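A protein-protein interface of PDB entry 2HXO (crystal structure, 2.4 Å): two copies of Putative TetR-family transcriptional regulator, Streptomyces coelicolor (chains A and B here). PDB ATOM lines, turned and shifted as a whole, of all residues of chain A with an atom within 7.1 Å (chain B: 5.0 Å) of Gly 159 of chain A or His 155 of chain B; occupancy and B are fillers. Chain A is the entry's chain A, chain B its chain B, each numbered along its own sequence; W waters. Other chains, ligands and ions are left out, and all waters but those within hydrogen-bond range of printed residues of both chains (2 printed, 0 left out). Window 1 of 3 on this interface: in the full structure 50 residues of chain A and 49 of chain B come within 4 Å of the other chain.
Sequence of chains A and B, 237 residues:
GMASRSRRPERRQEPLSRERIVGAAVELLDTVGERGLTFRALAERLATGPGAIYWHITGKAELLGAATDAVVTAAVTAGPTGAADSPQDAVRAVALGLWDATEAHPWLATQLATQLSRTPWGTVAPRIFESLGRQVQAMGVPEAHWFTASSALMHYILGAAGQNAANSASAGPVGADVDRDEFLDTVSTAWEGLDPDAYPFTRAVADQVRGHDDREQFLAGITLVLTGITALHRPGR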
ATOM      1  N   TRP A  99      24.488 -20.784 -16.212  1.00  0.00           N
ATOM      2  CA  TRP A  99      25.322 -21.033 -15.043  1.00  0.00           C
ATOM      3  C   TRP A  99      25.127 -19.954 -13.973  1.00  0.00           C
ATOM      4  O   TRP A  99      24.913 -20.265 -12.798  1.00  0.00           O
ATOM      5  CB  TRP A  99      26.796 -21.091 -15.455  1.00  0.00           C
ATOM      6  CG  TRP A  99      27.754 -21.058 -14.287  1.00  0.00           C
ATOM      7  CD1 TRP A  99      28.193 -19.945 -13.607  1.00  0.00           C
ATOM      8  CD2 TRP A  99      28.429 -22.176 -13.694  1.00  0.00           C
ATOM      9  NE1 TRP A  99      29.103 -20.308 -12.640  1.00  0.00           N
ATOM     10  CE2 TRP A  99      29.265 -21.669 -12.672  1.00  0.00           C
ATOM     11  CE3 TRP A  99      28.410 -23.554 -13.930  1.00  0.00           C
ATOM     12  CZ2 TRP A  99      30.079 -22.496 -11.892  1.00  0.00           C
ATOM     13  CZ3 TRP A  99      29.219 -24.378 -13.152  1.00  0.00           C
ATOM     14  CH2 TRP A  99      30.042 -23.845 -12.148  1.00  0.00           C
ATOM     15  N   LEU A 153      25.157 -30.286 -25.743  1.00  0.00           N
ATOM     16  CA  LEU A 153      25.498 -29.025 -25.077  1.00  0.00           C
ATOM     17  C   LEU A 153      24.584 -28.862 -23.860  1.00  0.00           C
ATOM     18  O   LEU A 153      25.043 -28.611 -22.746  1.00  0.00           O
ATOM     19  CB  LEU A 153      25.320 -27.849 -26.042  1.00  0.00           C
ATOM     20  CG  LEU A 153      26.435 -27.792 -27.083  1.00  0.00           C
ATOM     21  CD1 LEU A 153      26.024 -26.921 -28.263  1.00  0.00           C
ATOM     22  CD2 LEU A 153      27.711 -27.304 -26.407  1.00  0.00           C
ATOM     23  N   MET A 154      23.287 -29.049 -24.079  1.00  0.00           N
ATOM     24  CA  MET A 154      22.311 -28.943 -23.004  1.00  0.00           C
ATOM     25  C   MET A 154      22.617 -29.862 -21.816  1.00  0.00           C
ATOM     26  O   MET A 154      22.662 -29.420 -20.663  1.00  0.00           O
ATOM     27  CB  MET A 154      20.930 -29.276 -23.533  1.00  0.00           C
ATOM     28  CG  MET A 154      19.912 -29.363 -22.442  1.00  0.00           C
ATOM     29  SD  MET A 154      19.545 -27.604 -21.783  1.00  0.00           S
ATOM     30  CE  MET A 154      18.163 -27.177 -23.077  1.00  0.00           C
ATOM     31  N   HIS A 155      22.811 -31.146 -22.087  1.00  0.00           N
ATOM     32  CA  HIS A 155      23.092 -32.090 -21.016  1.00  0.00           C
ATOM     33  C   HIS A 155      24.360 -31.698 -20.277  1.00  0.00           C
ATOM     34  O   HIS A 155      24.465 -31.866 -19.057  1.00  0.00           O
ATOM     35  CB  HIS A 155      23.260 -33.520 -21.554  1.00  0.00           C
ATOM     36  CG  HIS A 155      21.976 -34.198 -21.918  1.00  0.00           C
ATOM     37  ND1 HIS A 155      21.695 -35.113 -22.874  1.00  0.00           N
ATOM     38  CD2 HIS A 155      20.805 -34.007 -21.217  1.00  0.00           C
ATOM     39  CE1 HIS A 155      20.373 -35.457 -22.732  1.00  0.00           C
ATOM     40  NE2 HIS A 155      19.858 -34.775 -21.726  1.00  0.00           N
ATOM     41  N   TYR A 156      25.352 -31.213 -21.012  1.00  0.00           N
ATOM     42  CA  TYR A 156      26.584 -30.803 -20.361  1.00  0.00           C
ATOM     43  C   TYR A 156      26.296 -29.630 -19.430  1.00  0.00           C
ATOM     44  O   TYR A 156      26.717 -29.615 -18.275  1.00  0.00           O
ATOM     45  CB  TYR A 156      27.648 -30.375 -21.365  1.00  0.00           C
ATOM     46  CG  TYR A 156      28.812 -29.767 -20.640  1.00  0.00           C
ATOM     47  CD1 TYR A 156      29.773 -30.571 -20.028  1.00  0.00           C
ATOM     48  CD2 TYR A 156      28.885 -28.382 -20.447  1.00  0.00           C
ATOM     49  CE1 TYR A 156      30.778 -30.013 -19.232  1.00  0.00           C
ATOM     50  CE2 TYR A 156      29.876 -27.816 -19.653  1.00  0.00           C
ATOM     51  CZ  TYR A 156      30.819 -28.631 -19.053  1.00  0.00           C
ATOM     52  OH  TYR A 156      31.820 -28.058 -18.307  1.00  0.00           O
ATOM     53  N   ILE A 157      25.568 -28.643 -19.933  1.00  0.00           N
ATOM     54  CA  ILE A 157      25.246 -27.478 -19.126  1.00  0.00           C
ATOM     55  C   ILE A 157      24.496 -27.836 -17.837  1.00  0.00           C
ATOM     56  O   ILE A 157      24.850 -27.361 -16.747  1.00  0.00           O
ATOM     57  CB  ILE A 157      24.444 -26.459 -19.956  1.00  0.00           C
ATOM     58  CG1 ILE A 157      25.357 -25.886 -21.046  1.00  0.00           C
ATOM     59  CG2 ILE A 157      23.910 -25.351 -19.056  1.00  0.00           C
ATOM     60  CD1 ILE A 157      24.658 -25.129 -22.143  1.00  0.00           C
ATOM     61  N   LEU A 158      23.469 -28.677 -17.956  1.00  0.00           N
ATOM     62  CA  LEU A 158      22.680 -29.108 -16.799  1.00  0.00           C
ATOM     63  C   LEU A 158      23.524 -29.852 -15.773  1.00  0.00           C
ATOM     64  O   LEU A 158      23.315 -29.734 -14.567  1.00  0.00           O
ATOM     65  CB  LEU A 158      21.547 -30.026 -17.248  1.00  0.00           C
ATOM     66  CG  LEU A 158      20.201 -29.419 -17.643  1.00  0.00           C
ATOM     67  CD1 LEU A 158      20.370 -28.201 -18.550  1.00  0.00           C
ATOM     68  CD2 LEU A 158      19.406 -30.497 -18.339  1.00  0.00           C
ATOM     69  N   GLY A 159      24.478 -30.631 -16.261  1.00  0.00           N
ATOM     70  CA  GLY A 159      25.329 -31.399 -15.372  1.00  0.00           C
ATOM     71  C   GLY A 159      26.337 -30.571 -14.597  1.00  0.00           C
ATOM     72  O   GLY A 159      26.536 -30.785 -13.399  1.00  0.00           O
ATOM     73  N   ALA A 160      26.999 -29.634 -15.267  1.00  0.00           N
ATOM     74  CA  ALA A 160      27.973 -28.801 -14.575  1.00  0.00           C
ATOM     75  C   ALA A 160      27.237 -27.756 -13.730  1.00  0.00           C
ATOM     76  O   ALA A 160      27.534 -27.585 -12.546  1.00  0.00           O
ATOM     77  CB  ALA A 160      28.904 -28.127 -15.581  1.00  0.00           C
ATOM     78  N   ALA A 161      26.266 -27.066 -14.326  1.00  0.00           N
ATOM     79  CA  ALA A 161      25.506 -26.058 -13.584  1.00  0.00           C
ATOM     80  C   ALA A 161      24.727 -26.702 -12.433  1.00  0.00           C
ATOM     81  O   ALA A 161      24.608 -26.125 -11.351  1.00  0.00           O
ATOM     82  CB  ALA A 161      24.545 -25.322 -14.516  1.00  0.00           C
ATOM     83  N   GLY A 162      24.194 -27.896 -12.677  1.00  0.00           N
ATOM     84  CA  GLY A 162      23.442 -28.596 -11.651  1.00  0.00           C
ATOM     85  C   GLY A 162      24.313 -28.876 -10.440  1.00  0.00           C
ATOM     86  O   GLY A 162      23.898 -28.659  -9.302  1.00  0.00           O
ATOM     87  N   GLN A 163      25.527 -29.358 -10.686  1.00  0.00           N
ATOM     88  CA  GLN A 163      26.459 -29.659  -9.609  1.00  0.00           C
ATOM     89  C   GLN A 163      26.867 -28.360  -8.922  1.00  0.00           C
ATOM     90  O   GLN A 163      27.016 -28.311  -7.702  1.00  0.00           O
ATOM     91  CB  GLN A 163      27.696 -30.373 -10.163  1.00  0.00           C
ATOM     92  CG  GLN A 163      28.603 -31.000  -9.107  1.00  0.00           C
ATOM     93  CD  GLN A 163      27.841 -31.891  -8.123  1.00  0.00           C
ATOM     94  OE1 GLN A 163      26.876 -32.567  -8.490  1.00  0.00           O
ATOM     95  NE2 GLN A 163      28.286 -31.903  -6.869  1.00  0.00           N
ATOM     96  N   ASN A 164      27.045 -27.306  -9.710  1.00  0.00           N
ATOM     97  CA  ASN A 164      27.415 -26.007  -9.162  1.00  0.00           C
ATOM     98  C   ASN A 164      26.350 -25.518  -8.171  1.00  0.00           C
ATOM     99  O   ASN A 164      26.679 -24.995  -7.102  1.00  0.00           O
ATOM    100  CB  ASN A 164      27.576 -24.986 -10.286  1.00  0.00           C
ATOM    101  CG  ASN A 164      27.704 -23.572  -9.767  1.00  0.00           C
ATOM    102  OD1 ASN A 164      28.635 -23.256  -9.028  1.00  0.00           O
ATOM    103  ND2 ASN A 164      26.761 -22.712 -10.148  1.00  0.00           N
ATOM    104  N   HIS A 212      40.742 -24.573  -7.588  1.00  0.00           N
ATOM    105  CA  HIS A 212      40.124 -24.924  -8.854  1.00  0.00           C
ATOM    106  C   HIS A 212      38.873 -24.071  -9.005  1.00  0.00           C
ATOM    107  O   HIS A 212      37.965 -24.151  -8.180  1.00  0.00           O
ATOM    108  CB  HIS A 212      39.761 -26.413  -8.855  1.00  0.00           C
ATOM    109  CG  HIS A 212      38.714 -26.782  -9.859  1.00  0.00           C
ATOM    110  ND1 HIS A 212      37.413 -27.076  -9.504  1.00  0.00           N
ATOM    111  CD2 HIS A 212      38.767 -26.879 -11.210  1.00  0.00           C
ATOM    112  CE1 HIS A 212      36.712 -27.340 -10.593  1.00  0.00           C
ATOM    113  NE2 HIS A 212      37.510 -27.229 -11.640  1.00  0.00           N
ATOM    114  N   ASP A 214      35.410 -23.214 -10.459  1.00  0.00           N
ATOM    115  CA  ASP A 214      34.288 -23.914 -11.067  1.00  0.00           C
ATOM    116  C   ASP A 214      33.859 -23.267 -12.385  1.00  0.00           C
ATOM    117  O   ASP A 214      33.682 -23.952 -13.388  1.00  0.00           O
ATOM    118  CB  ASP A 214      33.102 -23.937 -10.098  1.00  0.00           C
ATOM    119  CG  ASP A 214      33.439 -24.604  -8.777  1.00  0.00           C
ATOM    120  OD1 ASP A 214      33.647 -25.839  -8.769  1.00  0.00           O
ATOM    121  OD2 ASP A 214      33.500 -23.893  -7.748  1.00  0.00           O
ATOM    122  N   GLN A 217      36.123 -23.994 -15.138  1.00  0.00           N
ATOM    123  CA  GLN A 217      35.997 -25.400 -15.470  1.00  0.00           C
ATOM    124  C   GLN A 217      34.804 -25.518 -16.420  1.00  0.00           C
ATOM    125  O   GLN A 217      34.886 -26.140 -17.482  1.00  0.00           O
ATOM    126  CB  GLN A 217      35.733 -26.219 -14.203  1.00  0.00           C
ATOM    127  CG  GLN A 217      35.445 -27.688 -14.482  1.00  0.00           C
ATOM    128  CD  GLN A 217      36.590 -28.344 -15.217  1.00  0.00           C
ATOM    129  OE1 GLN A 217      37.726 -28.301 -14.748  1.00  0.00           O
ATOM    130  NE2 GLN A 217      36.304 -28.948 -16.381  1.00  0.00           N
ATOM    131  N   PHE A 218      33.699 -24.903 -16.015  1.00  0.00           N
ATOM    132  CA  PHE A 218      32.470 -24.892 -16.779  1.00  0.00           C
ATOM    133  C   PHE A 218      32.711 -24.485 -18.228  1.00  0.00           C
ATOM    134  O   PHE A 218      32.336 -25.213 -19.151  1.00  0.00           O
ATOM    135  CB  PHE A 218      31.477 -23.931 -16.131  1.00  0.00           C
ATOM    136  CG  PHE A 218      30.129 -23.908 -16.806  1.00  0.00           C
ATOM    137  CD1 PHE A 218      29.345 -25.060 -16.862  1.00  0.00           C
ATOM    138  CD2 PHE A 218      29.651 -22.741 -17.402  1.00  0.00           C
ATOM    139  CE1 PHE A 218      28.107 -25.057 -17.499  1.00  0.00           C
ATOM    140  CE2 PHE A 218      28.413 -22.728 -18.043  1.00  0.00           C
ATOM    141  CZ  PHE A 218      27.636 -23.899 -18.090  1.00  0.00           C
ATOM    142  N   GLY A 221      34.870 -27.006 -20.192  1.00  0.00           N
ATOM    143  CA  GLY A 221      34.110 -28.188 -20.576  1.00  0.00           C
ATOM    144  C   GLY A 221      33.220 -27.928 -21.785  1.00  0.00           C
ATOM    145  O   GLY A 221      33.158 -28.748 -22.707  1.00  0.00           O
ATOM    146  N   SER B 151      37.165 -33.845 -15.366  1.00  0.00           N
ATOM    147  CA  SER B 151      36.001 -33.208 -14.770  1.00  0.00           C
ATOM    148  C   SER B 151      34.900 -32.988 -15.789  1.00  0.00           C
ATOM    149  O   SER B 151      33.718 -33.062 -15.455  1.00  0.00           O
ATOM    150  CB  SER B 151      36.391 -31.862 -14.152  1.00  0.00           C
ATOM    151  OG  SER B 151      37.210 -32.052 -13.007  1.00  0.00           O
ATOM    152  N   ALA B 152      35.290 -32.701 -17.029  1.00  0.00           N
ATOM    153  CA  ALA B 152      34.323 -32.464 -18.095  1.00  0.00           C
ATOM    154  C   ALA B 152      33.560 -33.756 -18.369  1.00  0.00           C
ATOM    155  O   ALA B 152      32.341 -33.746 -18.522  1.00  0.00           O
ATOM    156  CB  ALA B 152      35.038 -31.995 -19.364  1.00  0.00           C
ATOM    157  N   LEU B 153      34.290 -34.865 -18.436  1.00  0.00           N
ATOM    158  CA  LEU B 153      33.670 -36.150 -18.678  1.00  0.00           C
ATOM    159  C   LEU B 153      32.686 -36.425 -17.559  1.00  0.00           C
ATOM    160  O   LEU B 153      31.542 -36.792 -17.820  1.00  0.00           O
ATOM    161  CB  LEU B 153      34.733 -37.250 -18.746  1.00  0.00           C
ATOM    162  CG  LEU B 153      35.413 -37.367 -20.113  1.00  0.00           C
ATOM    163  CD1 LEU B 153      36.659 -38.282 -20.058  1.00  0.00           C
ATOM    164  CD2 LEU B 153      34.368 -37.907 -21.091  1.00  0.00           C
ATOM    165  N   MET B 154      33.130 -36.208 -16.318  1.00  0.00           N
ATOM    166  CA  MET B 154      32.296 -36.433 -15.143  1.00  0.00           C
ATOM    167  C   MET B 154      31.030 -35.579 -15.153  1.00  0.00           C
ATOM    168  O   MET B 154      29.915 -36.089 -14.984  1.00  0.00           O
ATOM    169  CB  MET B 154      33.103 -36.167 -13.870  1.00  0.00           C
ATOM    170  CG  MET B 154      32.586 -36.936 -12.649  1.00  0.00           C
ATOM    171  SD  MET B 154      33.864 -37.126 -11.175  1.00  0.00           S
ATOM    172  CE  MET B 154      35.162 -38.242 -12.053  1.00  0.00           C
ATOM    173  N   HIS B 155      31.194 -34.283 -15.361  1.00  0.00           N
ATOM    174  CA  HIS B 155      30.050 -33.387 -15.394  1.00  0.00           C
ATOM    175  C   HIS B 155      29.100 -33.774 -16.510  1.00  0.00           C
ATOM    176  O   HIS B 155      27.888 -33.697 -16.345  1.00  0.00           O
ATOM    177  CB  HIS B 155      30.521 -31.945 -15.576  1.00  0.00           C
ATOM    178  CG  HIS B 155      31.231 -31.397 -14.377  1.00  0.00           C
ATOM    179  ND1 HIS B 155      31.995 -30.249 -14.422  1.00  0.00           N
ATOM    180  CD2 HIS B 155      31.274 -31.832 -13.095  1.00  0.00           C
ATOM    181  CE1 HIS B 155      32.477 -30.002 -13.216  1.00  0.00           C
ATOM    182  NE2 HIS B 155      32.055 -30.946 -12.393  1.00  0.00           N
ATOM    183  N   TYR B 156      29.645 -34.179 -17.650  1.00  0.00           N
ATOM    184  CA  TYR B 156      28.789 -34.583 -18.749  1.00  0.00           C
ATOM    185  C   TYR B 156      27.962 -35.797 -18.324  1.00  0.00           C
ATOM    186  O   TYR B 156      26.746 -35.807 -18.513  1.00  0.00           O
ATOM    187  CB  TYR B 156      29.604 -34.942 -19.994  1.00  0.00           C
ATOM    188  CG  TYR B 156      28.737 -35.549 -21.063  1.00  0.00           C
ATOM    189  CD1 TYR B 156      27.890 -34.751 -21.834  1.00  0.00           C
ATOM    190  CD2 TYR B 156      28.682 -36.929 -21.237  1.00  0.00           C
ATOM    191  CE1 TYR B 156      27.001 -35.314 -22.740  1.00  0.00           C
ATOM    192  CE2 TYR B 156      27.789 -37.509 -22.144  1.00  0.00           C
ATOM    193  CZ  TYR B 156      26.953 -36.697 -22.888  1.00  0.00           C
ATOM    194  OH  TYR B 156      26.045 -37.258 -23.755  1.00  0.00           O
ATOM    195  N   ILE B 157      28.630 -36.801 -17.746  1.00  0.00           N
ATOM    196  CA  ILE B 157      27.962 -38.034 -17.295  1.00  0.00           C
ATOM    197  C   ILE B 157      26.813 -37.743 -16.319  1.00  0.00           C
ATOM    198  O   ILE B 157      25.695 -38.229 -16.498  1.00  0.00           O
ATOM    199  CB  ILE B 157      28.939 -39.006 -16.558  1.00  0.00           C
ATOM    200  CG1 ILE B 157      30.195 -39.292 -17.389  1.00  0.00           C
ATOM    201  CG2 ILE B 157      28.212 -40.292 -16.200  1.00  0.00           C
ATOM    202  CD1 ILE B 157      29.939 -39.823 -18.733  1.00  0.00           C
ATOM    203  N   LEU B 158      27.102 -36.957 -15.286  1.00  0.00           N
ATOM    204  CA  LEU B 158      26.113 -36.607 -14.276  1.00  0.00           C
ATOM    205  C   LEU B 158      24.915 -35.878 -14.867  1.00  0.00           C
ATOM    206  O   LEU B 158      23.781 -36.069 -14.439  1.00  0.00           O
ATOM    207  CB  LEU B 158      26.768 -35.731 -13.205  1.00  0.00           C
ATOM    208  CG  LEU B 158      27.643 -36.392 -12.125  1.00  0.00           C
ATOM    209  CD1 LEU B 158      26.784 -36.688 -10.891  1.00  0.00           C
ATOM    210  CD2 LEU B 158      28.298 -37.666 -12.654  1.00  0.00           C
ATOM    211  N   GLY B 159      25.164 -35.030 -15.854  1.00  0.00           N
ATOM    212  CA  GLY B 159      24.073 -34.293 -16.456  1.00  0.00           C
ATOM    213  C   GLY B 159      23.145 -35.148 -17.296  1.00  0.00           C
ATOM    214  O   GLY B 159      21.927 -35.002 -17.211  1.00  0.00           O
HETATM  215  O   HOH W   1      23.905 -35.816 -24.751  1.00  0.00           O
HETATM  216  O   HOH W   2      33.609 -29.194 -16.588  1.00  0.00           O
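His 155 of chain A touches Gly 159 of chain B, and with the chains exchanged Gly 159 of chain A touches His 155 of chain B. Gly 159 of chain A touches its own counterpart, Gly 159 of chain B. Of the 7 pairs that touch across the chains among the printed residues, 3 have their exchanged pair printed and touching as well.
The side-chain amide oxygen (OE1) of Gln 217 of chain A lies close to a ring nitrogen (NE2) of His 212 of chain A (3.3 Å). A ring nitrogen (ND1) of His 155 of chain B sits close to the backbone carbonyl oxygen of Ser 151 of chain B (3.5 Å).
Water W2 lies within hydrogen-bond range of the side-chain amide nitrogen (NE2) of Gln 217 of chain A, the side-chain hydroxyl (OH) of Tyr 156 of chain A and a ring nitrogen (ND1) of His 155 of chain B. Water W1 lies within hydrogen-bond range of OH of Tyr 156 of chain B (2.8 Å) and ND1 of His 155 of chain A (3.0 Å).
Printed residues of chain A that touch a printed residue of chain B: His 155, Gly 159, Ala 160 and Gln 217. Hydrophobic or aromatic side chains of chain A that line the printed part of chain B: Ala 160. Of the 9 printed residues of chain B, 4 touch a printed residue of chain A. Among the printed residues, 7 pairs touch across the chains.
Of the printed residues of chain B, His 155 of chain A touches Gly 159 (3.6 Å). Gly 159 of chain A touches two residues of chain B. His 212 of chain A touches none of the printed residues of chain B. Printed residues of chain A within 4 Å of Ala 152 of chain B: Gln 217 (3.9 Å). Of chain A, only Gly 159 (3.6 Å), Ala 160 (3.9 Å) and Gln 217 (3.97 Å) come within 4 Å of His 155 of chain B. The nearest printed residue of chain B that does not touch Ala 160 of chain A is Gly 159 of chain B (5.6 Å).
Among the printed residues, merely in contact across the chains: Gly 159 of chain A with Gly 159 of chain B (3.3 Å), Gly 159 of chain A with His 155 of chain B (3.6 Å), His 155 of chain A with Gly 159 of chain B (3.6 Å), Gln 217 of chain A with Ser 151 of chain B (3.7 Å), Ala 160 of chain A with His 155 of chain B (3.9 Å), Gln 217 of chain A with Ala 152 of chain B (3.9 Å) and Gln 217 of chain A with His 155 of chain B (3.97 Å).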
